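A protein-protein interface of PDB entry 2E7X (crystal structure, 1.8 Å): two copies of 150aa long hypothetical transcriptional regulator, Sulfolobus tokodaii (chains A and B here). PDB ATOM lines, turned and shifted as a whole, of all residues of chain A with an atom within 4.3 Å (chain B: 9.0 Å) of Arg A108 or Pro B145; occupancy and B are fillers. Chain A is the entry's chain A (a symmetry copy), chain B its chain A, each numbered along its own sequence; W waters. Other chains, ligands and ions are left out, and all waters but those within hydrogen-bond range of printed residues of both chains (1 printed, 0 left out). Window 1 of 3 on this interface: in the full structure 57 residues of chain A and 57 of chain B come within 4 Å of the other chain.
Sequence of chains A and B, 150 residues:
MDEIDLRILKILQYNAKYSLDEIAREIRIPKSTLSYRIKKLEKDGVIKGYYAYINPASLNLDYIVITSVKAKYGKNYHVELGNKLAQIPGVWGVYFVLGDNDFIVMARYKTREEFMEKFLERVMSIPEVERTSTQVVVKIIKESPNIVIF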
ATOM      1  N   LEU A  61      24.346  15.779 -31.218  1.00  0.00           N
ATOM      2  CA  LEU A  61      24.357  14.385 -30.789  1.00  0.00           C
ATOM      3  C   LEU A  61      22.983  14.084 -30.192  1.00  0.00           C
ATOM      4  O   LEU A  61      22.803  14.102 -28.974  1.00  0.00           O
ATOM      5  CB  LEU A  61      25.471  14.164 -29.760  1.00  0.00           C
ATOM      6  CG  LEU A  61      26.887  14.359 -30.317  1.00  0.00           C
ATOM      7  CD1 LEU A  61      27.897  14.398 -29.174  1.00  0.00           C
ATOM      8  CD2 LEU A  61      27.216  13.232 -31.300  1.00  0.00           C
ATOM      9  N   TYR A  63      21.140  11.221 -31.128  1.00  0.00           N
ATOM     10  CA  TYR A  63      20.864   9.790 -31.117  1.00  0.00           C
ATOM     11  C   TYR A  63      21.694   9.179 -29.994  1.00  0.00           C
ATOM     12  O   TYR A  63      22.852   8.802 -30.185  1.00  0.00           O
ATOM     13  CB  TYR A  63      21.223   9.155 -32.461  1.00  0.00           C
ATOM     14  CG  TYR A  63      20.198   8.134 -32.891  1.00  0.00           C
ATOM     15  CD1 TYR A  63      19.002   8.532 -33.494  1.00  0.00           C
ATOM     16  CD2 TYR A  63      20.378   6.780 -32.618  1.00  0.00           C
ATOM     17  CE1 TYR A  63      18.009   7.605 -33.809  1.00  0.00           C
ATOM     18  CE2 TYR A  63      19.394   5.848 -32.924  1.00  0.00           C
ATOM     19  CZ  TYR A  63      18.214   6.266 -33.518  1.00  0.00           C
ATOM     20  OH  TYR A  63      17.237   5.343 -33.806  1.00  0.00           O
ATOM     21  N   ILE A  64      21.079   9.099 -28.819  1.00  0.00           N
ATOM     22  CA  ILE A  64      21.727   8.591 -27.614  1.00  0.00           C
ATOM     23  C   ILE A  64      21.264   7.170 -27.321  1.00  0.00           C
ATOM     24  O   ILE A  64      20.063   6.906 -27.246  1.00  0.00           O
ATOM     25  CB  ILE A  64      21.395   9.510 -26.417  1.00  0.00           C
ATOM     26  CG1 ILE A  64      21.734  10.962 -26.779  1.00  0.00           C
ATOM     27  CG2 ILE A  64      22.172   9.087 -25.184  1.00  0.00           C
ATOM     28  CD1 ILE A  64      23.190  11.173 -27.177  1.00  0.00           C
ATOM     29  N   GLY A  90      32.295   7.056 -31.037  1.00  0.00           N
ATOM     30  CA  GLY A  90      30.978   7.372 -30.506  1.00  0.00           C
ATOM     31  C   GLY A  90      30.687   6.696 -29.177  1.00  0.00           C
ATOM     32  O   GLY A  90      29.800   7.126 -28.432  1.00  0.00           O
ATOM     33  N   TRP A  92      31.424   5.992 -25.453  1.00  0.00           N
ATOM     34  CA  TRP A  92      32.163   6.604 -24.357  1.00  0.00           C
ATOM     35  C   TRP A  92      32.175   5.748 -23.098  1.00  0.00           C
ATOM     36  O   TRP A  92      32.983   5.969 -22.199  1.00  0.00           O
ATOM     37  CB  TRP A  92      31.629   8.010 -24.029  1.00  0.00           C
ATOM     38  CG  TRP A  92      30.185   8.109 -23.616  1.00  0.00           C
ATOM     39  CD1 TRP A  92      29.125   8.448 -24.410  1.00  0.00           C
ATOM     40  CD2 TRP A  92      29.654   7.936 -22.294  1.00  0.00           C
ATOM     41  NE1 TRP A  92      27.970   8.508 -23.663  1.00  0.00           N
ATOM     42  CE2 TRP A  92      28.266   8.199 -22.361  1.00  0.00           C
ATOM     43  CE3 TRP A  92      30.217   7.589 -21.057  1.00  0.00           C
ATOM     44  CZ2 TRP A  92      27.431   8.124 -21.240  1.00  0.00           C
ATOM     45  CZ3 TRP A  92      29.384   7.514 -19.937  1.00  0.00           C
ATOM     46  CH2 TRP A  92      28.004   7.783 -20.039  1.00  0.00           C
ATOM     47  N   ALA A 107      26.728   5.212 -25.878  1.00  0.00           N
ATOM     48  CA  ALA A 107      27.226   5.869 -27.086  1.00  0.00           C
ATOM     49  C   ALA A 107      26.344   7.032 -27.528  1.00  0.00           C
ATOM     50  O   ALA A 107      25.185   7.134 -27.124  1.00  0.00           O
ATOM     51  CB  ALA A 107      27.361   4.854 -28.213  1.00  0.00           C
ATOM     52  N   ARG A 108      26.912   7.915 -28.348  1.00  0.00           N
ATOM     53  CA  ARG A 108      26.195   9.082 -28.860  1.00  0.00           C
ATOM     54  C   ARG A 108      26.482   9.249 -30.348  1.00  0.00           C
ATOM     55  O   ARG A 108      27.620   9.071 -30.781  1.00  0.00           O
ATOM     56  CB  ARG A 108      26.664  10.370 -28.172  1.00  0.00           C
ATOM     57  CG  ARG A 108      26.805  10.355 -26.662  1.00  0.00           C
ATOM     58  CD  ARG A 108      27.033  11.793 -26.186  1.00  0.00           C
ATOM     59  NE  ARG A 108      27.241  11.915 -24.745  1.00  0.00           N
ATOM     60  CZ  ARG A 108      28.432  11.964 -24.156  1.00  0.00           C
ATOM     61  NH1 ARG A 108      29.543  11.901 -24.880  1.00  0.00           N
ATOM     62  NH2 ARG A 108      28.512  12.079 -22.838  1.00  0.00           N
ATOM     63  N   TYR A 109      25.452   9.601 -31.117  1.00  0.00           N
ATOM     64  CA  TYR A 109      25.586   9.838 -32.551  1.00  0.00           C
ATOM     65  C   TYR A 109      24.647  10.971 -32.944  1.00  0.00           C
ATOM     66  O   TYR A 109      23.753  11.336 -32.181  1.00  0.00           O
ATOM     67  CB  TYR A 109      25.258   8.567 -33.346  1.00  0.00           C
ATOM     68  CG  TYR A 109      26.228   7.443 -33.056  1.00  0.00           C
ATOM     69  CD1 TYR A 109      27.537   7.487 -33.532  1.00  0.00           C
ATOM     70  CD2 TYR A 109      25.870   6.393 -32.212  1.00  0.00           C
ATOM     71  CE1 TYR A 109      28.472   6.520 -33.163  1.00  0.00           C
ATOM     72  CE2 TYR A 109      26.792   5.422 -31.836  1.00  0.00           C
ATOM     73  CZ  TYR A 109      28.092   5.494 -32.311  1.00  0.00           C
ATOM     74  OH  TYR A 109      29.020   4.565 -31.896  1.00  0.00           O
ATOM     75  N   GLU A 143      22.844  13.701 -16.392  1.00  0.00           N
ATOM     76  CA  GLU A 143      24.093  13.104 -16.848  1.00  0.00           C
ATOM     77  C   GLU A 143      25.225  13.989 -16.359  1.00  0.00           C
ATOM     78  O   GLU A 143      25.712  14.855 -17.085  1.00  0.00           O
ATOM     79  CB  GLU A 143      24.157  12.975 -18.374  1.00  0.00           C
ATOM     80  CG  GLU A 143      25.377  12.178 -18.831  1.00  0.00           C
ATOM     81  CD  GLU A 143      25.424  11.949 -20.327  1.00  0.00           C
ATOM     82  OE1 GLU A 143      25.887  12.850 -21.058  1.00  0.00           O
ATOM     83  OE2 GLU A 143      24.994  10.866 -20.776  1.00  0.00           O
ATOM     84  N   PRO A 145      28.400  12.785 -14.708  1.00  0.00           N
ATOM     85  CA  PRO A 145      29.405  11.842 -14.207  1.00  0.00           C
ATOM     86  C   PRO A 145      30.558  12.517 -13.467  1.00  0.00           C
ATOM     87  O   PRO A 145      31.302  11.862 -12.739  1.00  0.00           O
ATOM     88  CB  PRO A 145      29.857  11.116 -15.474  1.00  0.00           C
ATOM     89  CG  PRO A 145      29.693  12.157 -16.538  1.00  0.00           C
ATOM     90  CD  PRO A 145      28.353  12.771 -16.180  1.00  0.00           C
ATOM     91  N   GLN B  13      38.184  19.158 -24.620  1.00  0.00           N
ATOM     92  CA  GLN B  13      37.444  18.041 -24.036  1.00  0.00           C
ATOM     93  C   GLN B  13      38.385  17.090 -23.289  1.00  0.00           C
ATOM     94  O   GLN B  13      37.949  16.306 -22.443  1.00  0.00           O
ATOM     95  CB  GLN B  13      36.702  17.276 -25.133  1.00  0.00           C
ATOM     96  CG  GLN B  13      37.596  16.367 -25.965  1.00  0.00           C
ATOM     97  CD  GLN B  13      36.869  15.741 -27.139  1.00  0.00           C
ATOM     98  OE1 GLN B  13      35.644  15.630 -27.138  1.00  0.00           O
ATOM     99  NE2 GLN B  13      37.625  15.314 -28.143  1.00  0.00           N
ATOM    100  N   TYR B  51      35.436  20.925 -15.630  1.00  0.00           N
ATOM    101  CA  TYR B  51      35.447  20.071 -14.452  1.00  0.00           C
ATOM    102  C   TYR B  51      36.766  19.336 -14.286  1.00  0.00           C
ATOM    103  O   TYR B  51      37.490  19.093 -15.251  1.00  0.00           O
ATOM    104  CB  TYR B  51      34.324  19.025 -14.554  1.00  0.00           C
ATOM    105  CG  TYR B  51      32.943  19.578 -14.870  1.00  0.00           C
ATOM    106  CD1 TYR B  51      32.022  18.825 -15.599  1.00  0.00           C
ATOM    107  CD2 TYR B  51      32.555  20.848 -14.442  1.00  0.00           C
ATOM    108  CE1 TYR B  51      30.752  19.324 -15.898  1.00  0.00           C
ATOM    109  CE2 TYR B  51      31.287  21.356 -14.737  1.00  0.00           C
ATOM    110  CZ  TYR B  51      30.394  20.590 -15.464  1.00  0.00           C
ATOM    111  OH  TYR B  51      29.148  21.095 -15.762  1.00  0.00           O
ATOM    112  N   TYR B  53      38.562  15.917 -13.527  1.00  0.00           N
ATOM    113  CA  TYR B  53      38.217  14.505 -13.609  1.00  0.00           C
ATOM    114  C   TYR B  53      38.851  13.816 -12.410  1.00  0.00           C
ATOM    115  O   TYR B  53      40.068  13.654 -12.345  1.00  0.00           O
ATOM    116  CB  TYR B  53      38.733  13.895 -14.917  1.00  0.00           C
ATOM    117  CG  TYR B  53      38.638  12.384 -14.979  1.00  0.00           C
ATOM    118  CD1 TYR B  53      37.450  11.724 -14.666  1.00  0.00           C
ATOM    119  CD2 TYR B  53      39.740  11.613 -15.348  1.00  0.00           C
ATOM    120  CE1 TYR B  53      37.361  10.333 -14.715  1.00  0.00           C
ATOM    121  CE2 TYR B  53      39.665  10.221 -15.401  1.00  0.00           C
ATOM    122  CZ  TYR B  53      38.472   9.587 -15.082  1.00  0.00           C
ATOM    123  OH  TYR B  53      38.393   8.212 -15.123  1.00  0.00           O
ATOM    124  N   TRP B  92      24.366   9.625 -10.796  1.00  0.00           N
ATOM    125  CA  TRP B  92      24.874  10.651 -11.697  1.00  0.00           C
ATOM    126  C   TRP B  92      24.197  10.632 -13.060  1.00  0.00           C
ATOM    127  O   TRP B  92      24.290  11.594 -13.818  1.00  0.00           O
ATOM    128  CB  TRP B  92      26.401  10.547 -11.870  1.00  0.00           C
ATOM    129  CG  TRP B  92      26.934   9.254 -12.425  1.00  0.00           C
ATOM    130  CD1 TRP B  92      27.457   8.209 -11.715  1.00  0.00           C
ATOM    131  CD2 TRP B  92      27.065   8.900 -13.810  1.00  0.00           C
ATOM    132  NE1 TRP B  92      27.913   7.232 -12.571  1.00  0.00           N
ATOM    133  CE2 TRP B  92      27.686   7.630 -13.863  1.00  0.00           C
ATOM    134  CE3 TRP B  92      26.720   9.534 -15.013  1.00  0.00           C
ATOM    135  CZ2 TRP B  92      27.969   6.980 -15.070  1.00  0.00           C
ATOM    136  CZ3 TRP B  92      27.002   8.886 -16.219  1.00  0.00           C
ATOM    137  CH2 TRP B  92      27.623   7.621 -16.235  1.00  0.00           C
ATOM    138  N   TYR B  95      18.282   8.122 -17.342  1.00  0.00           N
ATOM    139  CA  TYR B  95      17.851   8.156 -18.731  1.00  0.00           C
ATOM    140  C   TYR B  95      16.460   7.563 -18.941  1.00  0.00           C
ATOM    141  O   TYR B  95      16.189   6.452 -18.493  1.00  0.00           O
ATOM    142  CB  TYR B  95      18.850   7.363 -19.585  1.00  0.00           C
ATOM    143  CG  TYR B  95      20.288   7.820 -19.456  1.00  0.00           C
ATOM    144  CD1 TYR B  95      20.786   8.857 -20.244  1.00  0.00           C
ATOM    145  CD2 TYR B  95      21.152   7.207 -18.547  1.00  0.00           C
ATOM    146  CE1 TYR B  95      22.117   9.272 -20.137  1.00  0.00           C
ATOM    147  CE2 TYR B  95      22.481   7.616 -18.426  1.00  0.00           C
ATOM    148  CZ  TYR B  95      22.957   8.644 -19.223  1.00  0.00           C
ATOM    149  OH  TYR B  95      24.267   9.041 -19.111  1.00  0.00           O
ATOM    150  N   MET B 106      22.470   5.375 -13.487  1.00  0.00           N
ATOM    151  CA  MET B 106      23.889   5.124 -13.261  1.00  0.00           C
ATOM    152  C   MET B 106      24.225   5.686 -11.880  1.00  0.00           C
ATOM    153  O   MET B 106      23.915   6.843 -11.589  1.00  0.00           O
ATOM    154  CB  MET B 106      24.736   5.836 -14.323  1.00  0.00           C
ATOM    155  CG  MET B 106      24.258   5.649 -15.762  1.00  0.00           C
ATOM    156  SD  MET B 106      24.469   3.983 -16.438  1.00  0.00           S
ATOM    157  CE  MET B 106      26.166   4.021 -16.837  1.00  0.00           C
ATOM    158  N   ARG B 108      27.102   5.371  -8.178  1.00  0.00           N
ATOM    159  CA  ARG B 108      28.354   4.907  -7.583  1.00  0.00           C
ATOM    160  C   ARG B 108      28.266   5.002  -6.063  1.00  0.00           C
ATOM    161  O   ARG B 108      27.738   5.979  -5.535  1.00  0.00           O
ATOM    162  CB  ARG B 108      29.536   5.785  -8.012  1.00  0.00           C
ATOM    163  CG  ARG B 108      29.654   6.141  -9.483  1.00  0.00           C
ATOM    164  CD  ARG B 108      31.021   6.796  -9.710  1.00  0.00           C
ATOM    165  NE  ARG B 108      31.244   7.241 -11.082  1.00  0.00           N
ATOM    166  CZ  ARG B 108      31.034   8.479 -11.519  1.00  0.00           C
ATOM    167  NH1 ARG B 108      30.589   9.416 -10.690  1.00  0.00           N
ATOM    168  NH2 ARG B 108      31.272   8.781 -12.787  1.00  0.00           N
ATOM    169  N   ILE B 140      35.009  -1.578 -15.216  1.00  0.00           N
ATOM    170  CA  ILE B 140      34.741  -0.458 -16.102  1.00  0.00           C
ATOM    171  C   ILE B 140      35.813  -0.540 -17.176  1.00  0.00           C
ATOM    172  O   ILE B 140      36.992  -0.319 -16.900  1.00  0.00           O
ATOM    173  CB  ILE B 140      34.861   0.899 -15.375  1.00  0.00           C
ATOM    174  CG1 ILE B 140      33.755   1.028 -14.325  1.00  0.00           C
ATOM    175  CG2 ILE B 140      34.779   2.038 -16.390  1.00  0.00           C
ATOM    176  CD1 ILE B 140      33.797   2.332 -13.537  1.00  0.00           C
ATOM    177  N   LYS B 142      35.648   1.255 -20.045  1.00  0.00           N
ATOM    178  CA  LYS B 142      35.814   2.632 -20.492  1.00  0.00           C
ATOM    179  C   LYS B 142      34.722   3.531 -19.921  1.00  0.00           C
ATOM    180  O   LYS B 142      33.570   3.127 -19.822  1.00  0.00           O
ATOM    181  CB  LYS B 142      35.762   2.687 -22.025  1.00  0.00           C
ATOM    182  CG  LYS B 142      35.943   4.075 -22.623  1.00  0.00           C
ATOM    183  CD  LYS B 142      35.821   4.035 -24.142  1.00  0.00           C
ATOM    184  CE  LYS B 142      36.232   5.356 -24.772  1.00  0.00           C
ATOM    185  NZ  LYS B 142      36.122   5.313 -26.258  1.00  0.00           N
ATOM    186  N   GLU B 143      35.097   4.739 -19.521  1.00  0.00           N
ATOM    187  CA  GLU B 143      34.134   5.713 -19.020  1.00  0.00           C
ATOM    188  C   GLU B 143      34.728   7.092 -19.240  1.00  0.00           C
ATOM    189  O   GLU B 143      35.340   7.670 -18.343  1.00  0.00           O
ATOM    190  CB  GLU B 143      33.820   5.514 -17.534  1.00  0.00           C
ATOM    191  CG  GLU B 143      32.675   6.409 -17.064  1.00  0.00           C
ATOM    192  CD  GLU B 143      32.273   6.172 -15.624  1.00  0.00           C
ATOM    193  OE1 GLU B 143      32.925   6.735 -14.719  1.00  0.00           O
ATOM    194  OE2 GLU B 143      31.304   5.418 -15.393  1.00  0.00           O
ATOM    195  N   SER B 144      34.542   7.603 -20.452  1.00  0.00           N
ATOM    196  CA  SER B 144      35.057   8.909 -20.841  1.00  0.00           C
ATOM    197  C   SER B 144      33.940   9.741 -21.466  1.00  0.00           C
ATOM    198  O   SER B 144      34.005  10.099 -22.643  1.00  0.00           O
ATOM    199  CB  SER B 144      36.190   8.736 -21.856  1.00  0.00           C
ATOM    200  OG  SER B 144      37.232   7.933 -21.327  1.00  0.00           O
ATOM    201  N   PRO B 145      32.901  10.067 -20.680  1.00  0.00           N
ATOM    202  CA  PRO B 145      31.784  10.862 -21.199  1.00  0.00           C
ATOM    203  C   PRO B 145      32.199  12.246 -21.694  1.00  0.00           C
ATOM    204  O   PRO B 145      31.453  12.898 -22.422  1.00  0.00           O
ATOM    205  CB  PRO B 145      30.822  10.920 -20.012  1.00  0.00           C
ATOM    206  CG  PRO B 145      31.741  10.869 -18.830  1.00  0.00           C
ATOM    207  CD  PRO B 145      32.733   9.798 -19.242  1.00  0.00           C
ATOM    208  N   ASN B 146      33.391  12.680 -21.300  1.00  0.00           N
ATOM    209  CA  ASN B 146      33.914  13.983 -21.708  1.00  0.00           C
ATOM    210  C   ASN B 146      34.234  14.042 -23.203  1.00  0.00           C
ATOM    211  O   ASN B 146      34.274  15.125 -23.789  1.00  0.00           O
ATOM    212  CB  ASN B 146      35.181  14.312 -20.908  1.00  0.00           C
ATOM    213  CG  ASN B 146      36.256  13.254 -21.065  1.00  0.00           C
ATOM    214  OD1 ASN B 146      36.049  12.095 -20.710  1.00  0.00           O
ATOM    215  ND2 ASN B 146      37.408  13.645 -21.602  1.00  0.00           N
ATOM    216  N   ILE B 147      34.465  12.885 -23.818  1.00  0.00           N
ATOM    217  CA  ILE B 147      34.786  12.843 -25.242  1.00  0.00           C
ATOM    218  C   ILE B 147      33.533  12.901 -26.097  1.00  0.00           C
ATOM    219  O   ILE B 147      32.775  11.932 -26.177  1.00  0.00           O
ATOM    220  CB  ILE B 147      35.567  11.565 -25.615  1.00  0.00           C
ATOM    221  CG1 ILE B 147      36.756  11.395 -24.671  1.00  0.00           C
ATOM    222  CG2 ILE B 147      36.059  11.658 -27.061  1.00  0.00           C
ATOM    223  CD1 ILE B 147      37.552  12.666 -24.475  1.00  0.00           C
ATOM    224  N   VAL B 148      33.320  14.044 -26.739  1.00  0.00           N
ATOM    225  CA  VAL B 148      32.153  14.235 -27.586  1.00  0.00           C
ATOM    226  C   VAL B 148      32.559  14.320 -29.051  1.00  0.00           C
ATOM    227  O   VAL B 148      31.728  14.160 -29.943  1.00  0.00           O
ATOM    228  CB  VAL B 148      31.383  15.513 -27.178  1.00  0.00           C
ATOM    229  CG1 VAL B 148      30.694  15.295 -25.836  1.00  0.00           C
ATOM    230  CG2 VAL B 148      32.338  16.688 -27.083  1.00  0.00           C
ATOM    231  N   ILE B 149      33.846  14.565 -29.288  1.00  0.00           N
ATOM    232  CA  ILE B 149      34.389  14.656 -30.642  1.00  0.00           C
ATOM    233  C   ILE B 149      35.463  13.584 -30.800  1.00  0.00           C
ATOM    234  O   ILE B 149      36.522  13.662 -30.180  1.00  0.00           O
ATOM    235  CB  ILE B 149      35.021  16.040 -30.899  1.00  0.00           C
ATOM    236  CG1 ILE B 149      33.977  17.136 -30.685  1.00  0.00           C
ATOM    237  CG2 ILE B 149      35.576  16.105 -32.320  1.00  0.00           C
ATOM    238  CD1 ILE B 149      34.556  18.536 -30.659  1.00  0.00           C
ATOM    239  N   PHE B 150      35.178  12.577 -31.620  1.00  0.00           N
ATOM    240  CA  PHE B 150      36.115  11.483 -31.847  1.00  0.00           C
ATOM    241  C   PHE B 150      37.029  11.741 -33.043  1.00  0.00           C
ATOM    242  O   PHE B 150      38.053  11.031 -33.163  1.00  0.00           O
ATOM    243  CB  PHE B 150      35.354  10.166 -32.046  1.00  0.00           C
ATOM    244  CG  PHE B 150      34.657   9.680 -30.809  1.00  0.00           C
ATOM    245  CD1 PHE B 150      33.521  10.329 -30.332  1.00  0.00           C
ATOM    246  CD2 PHE B 150      35.160   8.598 -30.096  1.00  0.00           C
ATOM    247  CE1 PHE B 150      32.895   9.904 -29.158  1.00  0.00           C
ATOM    248  CE2 PHE B 150      34.545   8.166 -28.925  1.00  0.00           C
ATOM    249  CZ  PHE B 150      33.411   8.821 -28.451  1.00  0.00           C
ATOM    250  OXT PHE B 150      36.705  12.639 -33.849  1.00  0.00           O
HETATM  251  O   HOH W   1      30.083  10.180 -27.474  1.00  0.00           O
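NH2 of Arg A108 sits at hydrogen-bond distance from O of Pro B145, at 3.1 Å. N of Ser B144 lies within hydrogen-bond range of O of Trp A92. The guanidinium group of Arg B108 lies within hydrogen-bond range of the backbone carbonyl oxygen of Pro A145 (3.1 Å). The guanidinium group of Arg A108 is in hydrogen-bond range of the backbone carbonyl oxygen of Ile B147, 3.5 Å away. The side-chain carboxylate (OE2) of Glu A143 is in hydrogen-bond range of the side-chain hydroxyl (OH) of Tyr B95, 2.6 Å away.
The backbone NH (N) of Trp B92 sits at hydrogen-bond distance from the backbone carbonyl oxygen (O) of Met B106, 2.9 Å away. The side-chain amide oxygen of Asn B146 lies close to the backbone carbonyl oxygen of Ser B144 (3.4 Å). OE1 of Gln B13 is in hydrogen-bond range of N of Val B148 (2.8 Å). The guanidinium group of Arg B108 is in salt-bridge range of the side-chain carboxylate of Glu B143. The backbone NH (N) of Arg A108 is in hydrogen-bond range of the backbone carbonyl oxygen (O) of Gly A90. OE1 of Glu A143 is in salt-bridge range of NH2 of Arg A108, 3.3 Å away.
Val B148 touches Leu A61 (O to CD1, 3.9 Å). Phe B150 touches Gly A90. Trp B92 touches Trp A92. OH of Tyr B95 touches CZ2 of Trp A92, 3.9 Å away. O of Trp A92 touches CG of Lys B142 (3.5 Å). O of Trp A92 touches CA of Glu B143, 3.4 Å away. Trp A92 touches Pro B145. CG1 of Val B148 touches NH1 of Arg A108, 3.7 Å away. Glu A143 touches Trp B92 (CA to O, 3.4 Å). CE3 of Trp B92 touches CB of Pro A145, 3.5 Å away.
Of the printed residues of chain B, Leu A61 touches Val B148. Tyr A63 touches none of the printed residues of chain B. No residue of chain B comes within 4 Å of Tyr A109. Gln B13 touches none of the printed residues of chain A. Of the printed residues of chain A, Trp B92 touches Trp A92, Glu A143 and Pro A145. Printed residues of chain A within 4 Å of Lys B142: Trp A92. Of the printed residues of chain A, Glu B143 touches Trp A92 (3.4 Å). Pro B145 touches three residues of chain A. Printed residues of chain A within 4 Å of Val B148: Leu A61 (3.9 Å) and Arg A108 (3.7 Å). The nearest residue of chain B that does not touch Arg A108 is Asn B146 (5.2 Å). The nearest printed residue of chain A that does not touch Pro B145 is Glu A143 (5.4 Å). The nearest printed residue of chain B that does not touch Leu A61 is Ile B149 (6.0 Å).
Hydrophobic or aromatic side chains of chain B that line the printed part of chain A: Trp B92, Tyr B95, Pro B145, Val B148 and Phe B150. Along chain B the printed residues that touch a printed residue of chain A span positions 92 to 150. Among the printed residues, no Asp or Glu carboxylate lies within 4 Å of a Lys or Arg side-chain nitrogen of the other chain.
Trp A92 touches its own counterpart, Trp B92. Trp A92 touches Glu B143, and with the chains exchanged Glu A143 touches Trp B92. Trp A92 touches Pro B145, and with the chains exchanged Pro A145 touches Trp B92. Arg A108 touches Pro B145, and with the chains exchanged Pro A145 touches Arg B108. Of the 16 pairs that touch across the chains among the printed residues, 8 have their exchanged pair printed and touching as well.
Water W1 lies within hydrogen-bond range of NH1 of Arg A108, O of Gly A90 and O of Ile B147.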
